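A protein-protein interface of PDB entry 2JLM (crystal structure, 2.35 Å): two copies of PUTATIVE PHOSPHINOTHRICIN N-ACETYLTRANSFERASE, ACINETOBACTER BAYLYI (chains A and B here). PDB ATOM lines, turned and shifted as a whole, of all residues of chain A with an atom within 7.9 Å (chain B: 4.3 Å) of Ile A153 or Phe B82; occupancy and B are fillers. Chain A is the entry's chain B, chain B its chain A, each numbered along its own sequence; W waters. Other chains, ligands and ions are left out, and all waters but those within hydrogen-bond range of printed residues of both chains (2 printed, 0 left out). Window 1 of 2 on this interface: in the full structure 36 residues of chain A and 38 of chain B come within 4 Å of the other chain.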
ATOM      1  N   TYR A  39       3.137  19.149  16.766  1.00  0.00           N
ATOM      2  CA  TYR A  39       4.209  18.244  17.159  1.00  0.00           C
ATOM      3  C   TYR A  39       4.518  18.232  18.664  1.00  0.00           C
ATOM      4  O   TYR A  39       5.655  17.990  19.070  1.00  0.00           O
ATOM      5  CB  TYR A  39       5.451  18.475  16.297  1.00  0.00           C
ATOM      6  CG  TYR A  39       5.447  17.634  15.032  1.00  0.00           C
ATOM      7  CD1 TYR A  39       6.609  17.033  14.562  1.00  0.00           C
ATOM      8  CD2 TYR A  39       4.271  17.419  14.326  1.00  0.00           C
ATOM      9  CE1 TYR A  39       6.602  16.257  13.411  1.00  0.00           C
ATOM     10  CE2 TYR A  39       4.256  16.648  13.180  1.00  0.00           C
ATOM     11  CZ  TYR A  39       5.422  16.070  12.725  1.00  0.00           C
ATOM     12  OH  TYR A  39       5.403  15.303  11.576  1.00  0.00           O
ATOM     13  N   PHE A  82       9.398  31.259  10.415  1.00  0.00           N
ATOM     14  CA  PHE A  82       9.735  29.963   9.852  1.00  0.00           C
ATOM     15  C   PHE A  82      11.042  29.514  10.495  1.00  0.00           C
ATOM     16  O   PHE A  82      11.068  28.546  11.234  1.00  0.00           O
ATOM     17  CB  PHE A  82       9.883  30.058   8.327  1.00  0.00           C
ATOM     18  CG  PHE A  82      10.450  28.814   7.685  1.00  0.00           C
ATOM     19  CD1 PHE A  82      11.564  28.888   6.865  1.00  0.00           C
ATOM     20  CD2 PHE A  82       9.857  27.572   7.897  1.00  0.00           C
ATOM     21  CE1 PHE A  82      12.085  27.748   6.258  1.00  0.00           C
ATOM     22  CE2 PHE A  82      10.369  26.428   7.298  1.00  0.00           C
ATOM     23  CZ  PHE A  82      11.490  26.516   6.479  1.00  0.00           C
ATOM     24  N   ARG A  83      12.122  30.240  10.212  1.00  0.00           N
ATOM     25  CA  ARG A  83      13.399  30.032  10.880  1.00  0.00           C
ATOM     26  C   ARG A  83      13.839  31.364  11.481  1.00  0.00           C
ATOM     27  O   ARG A  83      13.699  32.421  10.856  1.00  0.00           O
ATOM     28  CB  ARG A  83      14.450  29.461   9.902  1.00  0.00           C
ATOM     29  CG  ARG A  83      14.170  28.006   9.500  1.00  0.00           C
ATOM     30  CD  ARG A  83      14.975  27.527   8.287  1.00  0.00           C
ATOM     31  NE  ARG A  83      16.426  27.668   8.459  1.00  0.00           N
ATOM     32  CZ  ARG A  83      17.186  26.860   9.199  1.00  0.00           C
ATOM     33  NH1 ARG A  83      16.641  25.848   9.864  1.00  0.00           N
ATOM     34  NH2 ARG A  83      18.495  27.074   9.288  1.00  0.00           N
ATOM     35  N   ALA A  84      14.357  31.321  12.701  1.00  0.00           N
ATOM     36  CA  ALA A  84      14.623  32.547  13.448  1.00  0.00           C
ATOM     37  C   ALA A  84      16.027  33.098  13.201  1.00  0.00           C
ATOM     38  O   ALA A  84      16.897  33.020  14.060  1.00  0.00           O
ATOM     39  CB  ALA A  84      14.372  32.330  14.940  1.00  0.00           C
ATOM     40  N   PHE A  85      16.230  33.629  12.001  1.00  0.00           N
ATOM     41  CA  PHE A  85      17.437  34.344  11.638  1.00  0.00           C
ATOM     42  C   PHE A  85      16.968  35.523  10.826  1.00  0.00           C
ATOM     43  O   PHE A  85      15.990  35.407  10.089  1.00  0.00           O
ATOM     44  CB  PHE A  85      18.368  33.478  10.791  1.00  0.00           C
ATOM     45  CG  PHE A  85      18.951  32.322  11.530  1.00  0.00           C
ATOM     46  CD1 PHE A  85      18.179  31.209  11.815  1.00  0.00           C
ATOM     47  CD2 PHE A  85      20.275  32.344  11.940  1.00  0.00           C
ATOM     48  CE1 PHE A  85      18.713  30.136  12.503  1.00  0.00           C
ATOM     49  CE2 PHE A  85      20.819  31.273  12.625  1.00  0.00           C
ATOM     50  CZ  PHE A  85      20.037  30.168  12.907  1.00  0.00           C
ATOM     51  N   CYS A 130       4.256  23.298   6.859  1.00  0.00           N
ATOM     52  CA  CYS A 130       4.861  22.026   7.216  1.00  0.00           C
ATOM     53  C   CYS A 130       3.737  21.033   7.451  1.00  0.00           C
ATOM     54  O   CYS A 130       2.885  21.241   8.311  1.00  0.00           O
ATOM     55  CB  CYS A 130       5.747  22.163   8.461  1.00  0.00           C
ATOM     56  SG  CYS A 130       6.857  20.750   8.727  1.00  0.00           S
ATOM     57  N   ILE A 131       3.732  19.963   6.662  1.00  0.00           N
ATOM     58  CA  ILE A 131       2.620  19.020   6.637  1.00  0.00           C
ATOM     59  C   ILE A 131       3.136  17.602   6.798  1.00  0.00           C
ATOM     60  O   ILE A 131       4.121  17.237   6.157  1.00  0.00           O
ATOM     61  CB  ILE A 131       1.936  19.098   5.257  1.00  0.00           C
ATOM     62  CG1 ILE A 131       1.612  20.556   4.916  1.00  0.00           C
ATOM     63  CG2 ILE A 131       0.706  18.197   5.190  1.00  0.00           C
ATOM     64  CD1 ILE A 131       1.007  20.742   3.526  1.00  0.00           C
ATOM     65  N   ALA A 133       3.691  14.279   5.608  1.00  0.00           N
ATOM     66  CA  ALA A 133       3.749  13.899   4.201  1.00  0.00           C
ATOM     67  C   ALA A 133       2.670  12.898   3.802  1.00  0.00           C
ATOM     68  O   ALA A 133       2.436  12.684   2.613  1.00  0.00           O
ATOM     69  CB  ALA A 133       5.100  13.355   3.862  1.00  0.00           C
ATOM     70  N   HIS A 149       5.551  21.892  -3.697  1.00  0.00           N
ATOM     71  CA  HIS A 149       6.288  20.999  -2.816  1.00  0.00           C
ATOM     72  C   HIS A 149       7.766  21.370  -2.828  1.00  0.00           C
ATOM     73  O   HIS A 149       8.438  21.194  -3.836  1.00  0.00           O
ATOM     74  CB  HIS A 149       6.100  19.545  -3.258  1.00  0.00           C
ATOM     75  CG  HIS A 149       6.811  18.550  -2.394  1.00  0.00           C
ATOM     76  ND1 HIS A 149       7.612  17.558  -2.912  1.00  0.00           N
ATOM     77  CD2 HIS A 149       6.852  18.400  -1.049  1.00  0.00           C
ATOM     78  CE1 HIS A 149       8.111  16.835  -1.925  1.00  0.00           C
ATOM     79  NE2 HIS A 149       7.664  17.326  -0.784  1.00  0.00           N
ATOM     80  N   SER A 150       8.263  21.882  -1.704  1.00  0.00           N
ATOM     81  CA  SER A 150       9.650  22.320  -1.616  1.00  0.00           C
ATOM     82  C   SER A 150      10.543  21.126  -1.352  1.00  0.00           C
ATOM     83  O   SER A 150      11.681  21.063  -1.825  1.00  0.00           O
ATOM     84  CB  SER A 150       9.828  23.347  -0.496  1.00  0.00           C
ATOM     85  OG  SER A 150       9.008  24.477  -0.710  1.00  0.00           O
ATOM     86  N   GLY A 151      10.023  20.186  -0.571  1.00  0.00           N
ATOM     87  CA  GLY A 151      10.730  18.956  -0.298  1.00  0.00           C
ATOM     88  C   GLY A 151      10.221  18.318   0.967  1.00  0.00           C
ATOM     89  O   GLY A 151       9.330  18.847   1.631  1.00  0.00           O
ATOM     90  N   THR A 152      10.825  17.187   1.313  1.00  0.00           N
ATOM     91  CA  THR A 152      10.385  16.394   2.449  1.00  0.00           C
ATOM     92  C   THR A 152      11.575  15.866   3.244  1.00  0.00           C
ATOM     93  O   THR A 152      12.512  15.298   2.691  1.00  0.00           O
ATOM     94  CB  THR A 152       9.524  15.224   1.972  1.00  0.00           C
ATOM     95  OG1 THR A 152       8.354  15.743   1.324  1.00  0.00           O
ATOM     96  CG2 THR A 152       9.114  14.339   3.156  1.00  0.00           C
ATOM     97  N   ILE A 153      11.549  16.092   4.546  1.00  0.00           N
ATOM     98  CA  ILE A 153      12.574  15.554   5.409  1.00  0.00           C
ATOM     99  C   ILE A 153      12.034  14.290   6.044  1.00  0.00           C
ATOM    100  O   ILE A 153      11.136  14.339   6.881  1.00  0.00           O
ATOM    101  CB  ILE A 153      12.983  16.554   6.493  1.00  0.00           C
ATOM    102  CG1 ILE A 153      13.554  17.810   5.831  1.00  0.00           C
ATOM    103  CG2 ILE A 153      13.980  15.909   7.440  1.00  0.00           C
ATOM    104  CD1 ILE A 153      13.808  18.961   6.774  1.00  0.00           C
ATOM    105  N   GLN A 154      12.586  13.157   5.626  1.00  0.00           N
ATOM    106  CA  GLN A 154      12.118  11.858   6.079  1.00  0.00           C
ATOM    107  C   GLN A 154      12.412  11.590   7.553  1.00  0.00           C
ATOM    108  O   GLN A 154      13.512  11.854   8.047  1.00  0.00           O
ATOM    109  CB  GLN A 154      12.717  10.758   5.193  1.00  0.00           C
ATOM    110  CG  GLN A 154      12.473  11.013   3.715  1.00  0.00           C
ATOM    111  CD  GLN A 154      12.915   9.860   2.844  1.00  0.00           C
ATOM    112  OE1 GLN A 154      12.437   8.734   2.994  1.00  0.00           O
ATOM    113  NE2 GLN A 154      13.824  10.136   1.917  1.00  0.00           N
ATOM    114  N   GLN A 155      11.397  11.092   8.244  1.00  0.00           N
ATOM    115  CA  GLN A 155      11.507  10.653   9.628  1.00  0.00           C
ATOM    116  C   GLN A 155      12.032  11.753  10.538  1.00  0.00           C
ATOM    117  O   GLN A 155      12.677  11.485  11.553  1.00  0.00           O
ATOM    118  CB  GLN A 155      12.367   9.390   9.705  1.00  0.00           C
ATOM    119  CG  GLN A 155      12.048   8.383   8.584  1.00  0.00           C
ATOM    120  CD  GLN A 155      12.714   7.026   8.784  1.00  0.00           C
ATOM    121  OE1 GLN A 155      13.246   6.728   9.855  1.00  0.00           O
ATOM    122  NE2 GLN A 155      12.699   6.206   7.743  1.00  0.00           N
ATOM    123  N   ALA A 156      11.744  12.994  10.167  1.00  0.00           N
ATOM    124  CA  ALA A 156      12.129  14.147  10.978  1.00  0.00           C
ATOM    125  C   ALA A 156      11.368  14.197  12.300  1.00  0.00           C
ATOM    126  O   ALA A 156      11.861  14.742  13.291  1.00  0.00           O
ATOM    127  CB  ALA A 156      11.925  15.431  10.202  1.00  0.00           C
ATOM    128  N   GLY A 157      10.170  13.624  12.322  1.00  0.00           N
ATOM    129  CA  GLY A 157       9.356  13.647  13.529  1.00  0.00           C
ATOM    130  C   GLY A 157       9.128  12.285  14.161  1.00  0.00           C
ATOM    131  O   GLY A 157       9.325  11.247  13.536  1.00  0.00           O
ATOM    132  N   LEU A 164       7.873  10.125  11.439  1.00  0.00           N
ATOM    133  CA  LEU A 164       6.969  10.874  10.569  1.00  0.00           C
ATOM    134  C   LEU A 164       7.770  11.707   9.588  1.00  0.00           C
ATOM    135  O   LEU A 164       8.779  12.302   9.959  1.00  0.00           O
ATOM    136  CB  LEU A 164       6.096  11.795  11.416  1.00  0.00           C
ATOM    137  CG  LEU A 164       5.276  11.074  12.482  1.00  0.00           C
ATOM    138  CD1 LEU A 164       4.687  12.071  13.467  1.00  0.00           C
ATOM    139  CD2 LEU A 164       4.183  10.236  11.832  1.00  0.00           C
ATOM    140  N   ASP A 165       7.321  11.747   8.337  1.00  0.00           N
ATOM    141  CA  ASP A 165       7.987  12.527   7.308  1.00  0.00           C
ATOM    142  C   ASP A 165       7.391  13.935   7.265  1.00  0.00           C
ATOM    143  O   ASP A 165       6.180  14.098   7.213  1.00  0.00           O
ATOM    144  CB  ASP A 165       7.858  11.841   5.945  1.00  0.00           C
ATOM    145  CG  ASP A 165       8.660  10.546   5.859  1.00  0.00           C
ATOM    146  OD1 ASP A 165       8.532   9.834   4.845  1.00  0.00           O
ATOM    147  OD2 ASP A 165       9.421  10.238   6.805  1.00  0.00           O
ATOM    148  N   ALA A 166       8.246  14.949   7.308  1.00  0.00           N
ATOM    149  CA  ALA A 166       7.781  16.329   7.299  1.00  0.00           C
ATOM    150  C   ALA A 166       7.911  16.939   5.909  1.00  0.00           C
ATOM    151  O   ALA A 166       9.015  17.120   5.381  1.00  0.00           O
ATOM    152  CB  ALA A 166       8.529  17.163   8.343  1.00  0.00           C
ATOM    153  N   ALA A 167       6.765  17.222   5.304  1.00  0.00           N
ATOM    154  CA  ALA A 167       6.721  17.791   3.969  1.00  0.00           C
ATOM    155  C   ALA A 167       6.621  19.316   4.061  1.00  0.00           C
ATOM    156  O   ALA A 167       5.920  19.853   4.923  1.00  0.00           O
ATOM    157  CB  ALA A 167       5.537  17.216   3.200  1.00  0.00           C
ATOM    158  N   PHE A 168       7.320  20.012   3.178  1.00  0.00           N
ATOM    159  CA  PHE A 168       7.268  21.467   3.165  1.00  0.00           C
ATOM    160  C   PHE A 168       6.721  21.953   1.852  1.00  0.00           C
ATOM    161  O   PHE A 168       7.216  21.568   0.790  1.00  0.00           O
ATOM    162  CB  PHE A 168       8.654  22.074   3.394  1.00  0.00           C
ATOM    163  CG  PHE A 168       9.206  21.785   4.747  1.00  0.00           C
ATOM    164  CD1 PHE A 168       9.859  20.588   4.995  1.00  0.00           C
ATOM    165  CD2 PHE A 168       9.047  22.694   5.789  1.00  0.00           C
ATOM    166  CE1 PHE A 168      10.371  20.308   6.257  1.00  0.00           C
ATOM    167  CE2 PHE A 168       9.545  22.424   7.051  1.00  0.00           C
ATOM    168  CZ  PHE A 168      10.213  21.229   7.288  1.00  0.00           C
ATOM    169  N   GLY B  80      22.186  21.937  16.966  1.00  0.00           N
ATOM    170  CA  GLY B  80      21.202  22.477  17.884  1.00  0.00           C
ATOM    171  C   GLY B  80      19.840  21.981  17.437  1.00  0.00           C
ATOM    172  O   GLY B  80      19.739  21.118  16.575  1.00  0.00           O
ATOM    173  N   SER B  81      18.787  22.531  18.019  1.00  0.00           N
ATOM    174  CA  SER B  81      17.439  22.166  17.634  1.00  0.00           C
ATOM    175  C   SER B  81      17.189  22.519  16.166  1.00  0.00           C
ATOM    176  O   SER B  81      17.559  23.597  15.718  1.00  0.00           O
ATOM    177  CB  SER B  81      16.447  22.903  18.540  1.00  0.00           C
ATOM    178  OG  SER B  81      15.276  23.250  17.831  1.00  0.00           O
ATOM    179  N   PHE B  82      16.564  21.610  15.422  1.00  0.00           N
ATOM    180  CA  PHE B  82      16.122  21.891  14.054  1.00  0.00           C
ATOM    181  C   PHE B  82      14.788  22.655  14.020  1.00  0.00           C
ATOM    182  O   PHE B  82      14.696  23.751  13.459  1.00  0.00           O
ATOM    183  CB  PHE B  82      16.006  20.590  13.256  1.00  0.00           C
ATOM    184  CG  PHE B  82      15.341  20.751  11.918  1.00  0.00           C
ATOM    185  CD1 PHE B  82      14.226  20.005  11.595  1.00  0.00           C
ATOM    186  CD2 PHE B  82      15.835  21.651  10.984  1.00  0.00           C
ATOM    187  CE1 PHE B  82      13.618  20.141  10.362  1.00  0.00           C
ATOM    188  CE2 PHE B  82      15.235  21.790   9.752  1.00  0.00           C
ATOM    189  CZ  PHE B  82      14.122  21.034   9.441  1.00  0.00           C
ATOM    190  N   ARG B  83      13.751  22.066  14.605  1.00  0.00           N
ATOM    191  CA  ARG B  83      12.483  22.773  14.813  1.00  0.00           C
ATOM    192  C   ARG B  83      12.110  22.595  16.286  1.00  0.00           C
ATOM    193  O   ARG B  83      12.293  21.519  16.851  1.00  0.00           O
ATOM    194  CB  ARG B  83      11.368  22.239  13.888  1.00  0.00           C
ATOM    195  CG  ARG B  83      11.505  22.627  12.407  1.00  0.00           C
ATOM    196  CD  ARG B  83      10.587  21.787  11.455  1.00  0.00           C
ATOM    197  NE  ARG B  83       9.149  21.995  11.690  1.00  0.00           N
ATOM    198  CZ  ARG B  83       8.476  23.123  11.430  1.00  0.00           C
ATOM    199  NH1 ARG B  83       9.082  24.187  10.915  1.00  0.00           N
ATOM    200  NH2 ARG B  83       7.180  23.188  11.700  1.00  0.00           N
ATOM    201  N   THR B  91      15.776  14.968  15.909  1.00  0.00           N
ATOM    202  CA  THR B  91      16.304  15.645  14.746  1.00  0.00           C
ATOM    203  C   THR B  91      17.099  16.848  15.221  1.00  0.00           C
ATOM    204  O   THR B  91      16.600  17.666  15.995  1.00  0.00           O
ATOM    205  CB  THR B  91      15.158  16.126  13.828  1.00  0.00           C
ATOM    206  OG1 THR B  91      14.431  14.992  13.332  1.00  0.00           O
ATOM    207  CG2 THR B  91      15.705  16.936  12.651  1.00  0.00           C
ATOM    208  N   VAL B  92      18.338  16.959  14.766  1.00  0.00           N
ATOM    209  CA  VAL B  92      19.143  18.133  15.092  1.00  0.00           C
ATOM    210  C   VAL B  92      19.553  18.821  13.807  1.00  0.00           C
ATOM    211  O   VAL B  92      19.623  18.191  12.744  1.00  0.00           O
ATOM    212  CB  VAL B  92      20.408  17.767  15.880  1.00  0.00           C
ATOM    213  CG1 VAL B  92      20.036  17.085  17.139  1.00  0.00           C
ATOM    214  CG2 VAL B  92      21.333  16.895  15.036  1.00  0.00           C
ATOM    215  N   GLU B  93      19.792  20.123  13.899  1.00  0.00           N
ATOM    216  CA  GLU B  93      20.363  20.869  12.785  1.00  0.00           C
ATOM    217  C   GLU B  93      21.824  21.172  13.094  1.00  0.00           C
ATOM    218  O   GLU B  93      22.144  21.735  14.141  1.00  0.00           O
ATOM    219  CB  GLU B  93      19.609  22.185  12.565  1.00  0.00           C
ATOM    220  CG  GLU B  93      20.260  23.024  11.491  1.00  0.00           C
ATOM    221  CD  GLU B  93      19.447  24.230  11.094  1.00  0.00           C
ATOM    222  OE1 GLU B  93      18.276  24.326  11.502  1.00  0.00           O
ATOM    223  OE2 GLU B  93      19.992  25.092  10.372  1.00  0.00           O
ATOM    224  N   VAL B 128      20.169  17.483  10.050  1.00  0.00           N
ATOM    225  CA  VAL B 128      19.791  18.336   8.925  1.00  0.00           C
ATOM    226  C   VAL B 128      20.789  19.466   8.742  1.00  0.00           C
ATOM    227  O   VAL B 128      21.093  20.198   9.681  1.00  0.00           O
ATOM    228  CB  VAL B 128      18.393  18.975   9.135  1.00  0.00           C
ATOM    229  CG1 VAL B 128      18.061  19.938   7.981  1.00  0.00           C
ATOM    230  CG2 VAL B 128      17.338  17.909   9.276  1.00  0.00           C
ATOM    231  N   SER B 150      16.911  16.798   0.776  1.00  0.00           N
ATOM    232  CA  SER B 150      15.489  16.703   1.136  1.00  0.00           C
ATOM    233  C   SER B 150      14.614  17.699   0.381  1.00  0.00           C
ATOM    234  O   SER B 150      13.461  17.402   0.074  1.00  0.00           O
ATOM    235  CB  SER B 150      15.300  16.926   2.640  1.00  0.00           C
ATOM    236  OG  SER B 150      16.142  16.085   3.402  1.00  0.00           O
ATOM    237  N   PHE B 168      17.844  21.966   2.155  1.00  0.00           N
ATOM    238  CA  PHE B 168      17.888  21.107   3.328  1.00  0.00           C
ATOM    239  C   PHE B 168      18.451  19.737   2.977  1.00  0.00           C
ATOM    240  O   PHE B 168      17.835  18.989   2.218  1.00  0.00           O
ATOM    241  CB  PHE B 168      16.500  21.009   3.954  1.00  0.00           C
ATOM    242  CG  PHE B 168      16.038  22.304   4.553  1.00  0.00           C
ATOM    243  CD1 PHE B 168      15.243  23.172   3.831  1.00  0.00           C
ATOM    244  CD2 PHE B 168      16.451  22.680   5.820  1.00  0.00           C
ATOM    245  CE1 PHE B 168      14.842  24.376   4.376  1.00  0.00           C
ATOM    246  CE2 PHE B 168      16.052  23.885   6.369  1.00  0.00           C
ATOM    247  CZ  PHE B 168      15.249  24.730   5.650  1.00  0.00           C
ATOM    248  N   GLN B 170      19.771  16.094   4.602  1.00  0.00           N
ATOM    249  CA  GLN B 170      19.561  15.296   5.795  1.00  0.00           C
ATOM    250  C   GLN B 170      20.357  14.015   5.732  1.00  0.00           C
ATOM    251  O   GLN B 170      20.638  13.490   4.654  1.00  0.00           O
ATOM    252  CB  GLN B 170      18.074  14.956   5.980  1.00  0.00           C
ATOM    253  CG  GLN B 170      17.599  13.754   5.146  1.00  0.00           C
ATOM    254  CD  GLN B 170      16.137  13.428   5.377  1.00  0.00           C
ATOM    255  OE1 GLN B 170      15.273  13.819   4.589  1.00  0.00           O
ATOM    256  NE2 GLN B 170      15.847  12.710   6.468  1.00  0.00           N
HETATM  257  O   HOH W   1      13.780  12.426  14.040  1.00  0.00           O
HETATM  258  O   HOH W   2      14.139  24.981  10.643  1.00  0.00           O
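The backbone carbonyl oxygen of Ala A156 is in hydrogen-bond range of the side-chain hydroxyl of Thr B91 (2.6 Å).
The side-chain carboxylate of Glu B93 lies within salt-bridge range of the guanidinium group of Arg A83, at 2.7 Å.
The backbone NH of Thr A152 lies within hydrogen-bond range of the backbone carbonyl oxygen of Ser B150 (2.9 Å).
The backbone carbonyl oxygen of Gln A154 sits at hydrogen-bond distance from the side-chain amide nitrogen of Gln B170, at 2.9 Å.
The backbone carbonyl oxygen of Glu B93 lies within hydrogen-bond range of the backbone NH of Gly B80, 2.8 Å away.
The backbone carbonyl oxygen (O) of Phe B168 is in hydrogen-bond range of the backbone NH (N) of Ser B150, 2.8 Å away.
OG of Ser B150 lies within hydrogen-bond range of OE1 of Gln B170 (2.7 Å).
The backbone carbonyl oxygen (O) of Gly A151 sits close to a ring nitrogen (NE2) of His A149 (3.3 Å).
N of Ile A153 is in hydrogen-bond range of O of Ala A166 (2.9 Å).
The backbone carbonyl oxygen (O) of Leu A164 sits at hydrogen-bond distance from the backbone NH (N) of Ala A156, 3.1 Å away.
CD of Arg A83 touches CZ of Phe B168, 3.9 Å away.
Cys A130 touches Arg B83.
Gly A151 touches Ser B150 (CA to O, 3.2 Å).
OE1 of Gln B170 touches O of Thr A152, 3.7 Å away.
Ile A153 touches Phe B82 (CD1 to CZ, 3.4 Å).
CG1 of Ile A153 touches CB of Ser B150, at 3.7 Å.
Ile A153 touches Gln B170 (CA to OE1, 3.3 Å).
Of the printed residues of chain B, Arg A83 touches Glu B93 and Phe B168.
Asp A165 touches none of the printed residues of chain B.
No residue of chain A comes within 4 Å of Ser B81.
Of chain A, only Ile A153 comes within 4 Å of Phe B82.
Val B92 touches none of the printed residues of chain A.
Printed residues of chain A within 4 Å of Glu B93: Arg A83.
Hydrophobic or aromatic side chains of chain B within 4 Å of the printed part of chain A: Phe B82 and Phe B168.
Of the 22 printed residues of chain A, 7 touch a printed residue of chain B.
Printed residues of chain A that touch a printed residue of chain B: Arg A83, Cys A130, Gly A151, Thr A152, Ile A153, Gln A154 and Ala A156.
Hydrophobic or aromatic side chains of chain A within 4 Å of the printed part of chain B: Ile A153.
Along chain A the printed residues that touch a printed residue of chain B span positions 83 to 156.
Among the printed residues, 11 pairs touch across the chains.
Among the printed residues, Asp or Glu carboxylates within 4 Å of a Lys or Arg side-chain nitrogen of the other chain: Arg A83 with Glu B93.
Arg A83 touches Phe B168, but with the chains exchanged Phe A168 does not touch Arg B83 (4.2 Å).
Positions printed for both chains: 82, 83, 150 and 168.
Of the 11 pairs that touch across the chains among the printed residues, none has its exchanged pair printed and touching as well.
Water W1 lies within hydrogen-bond range of OG1 of Thr B91 (2.7 Å), O of Gln A155 (2.9 Å) and O of Ala A156 (3.1 Å).
Water W2 lies within hydrogen-bond range of NH1 of Arg A83 and O of Phe B82.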
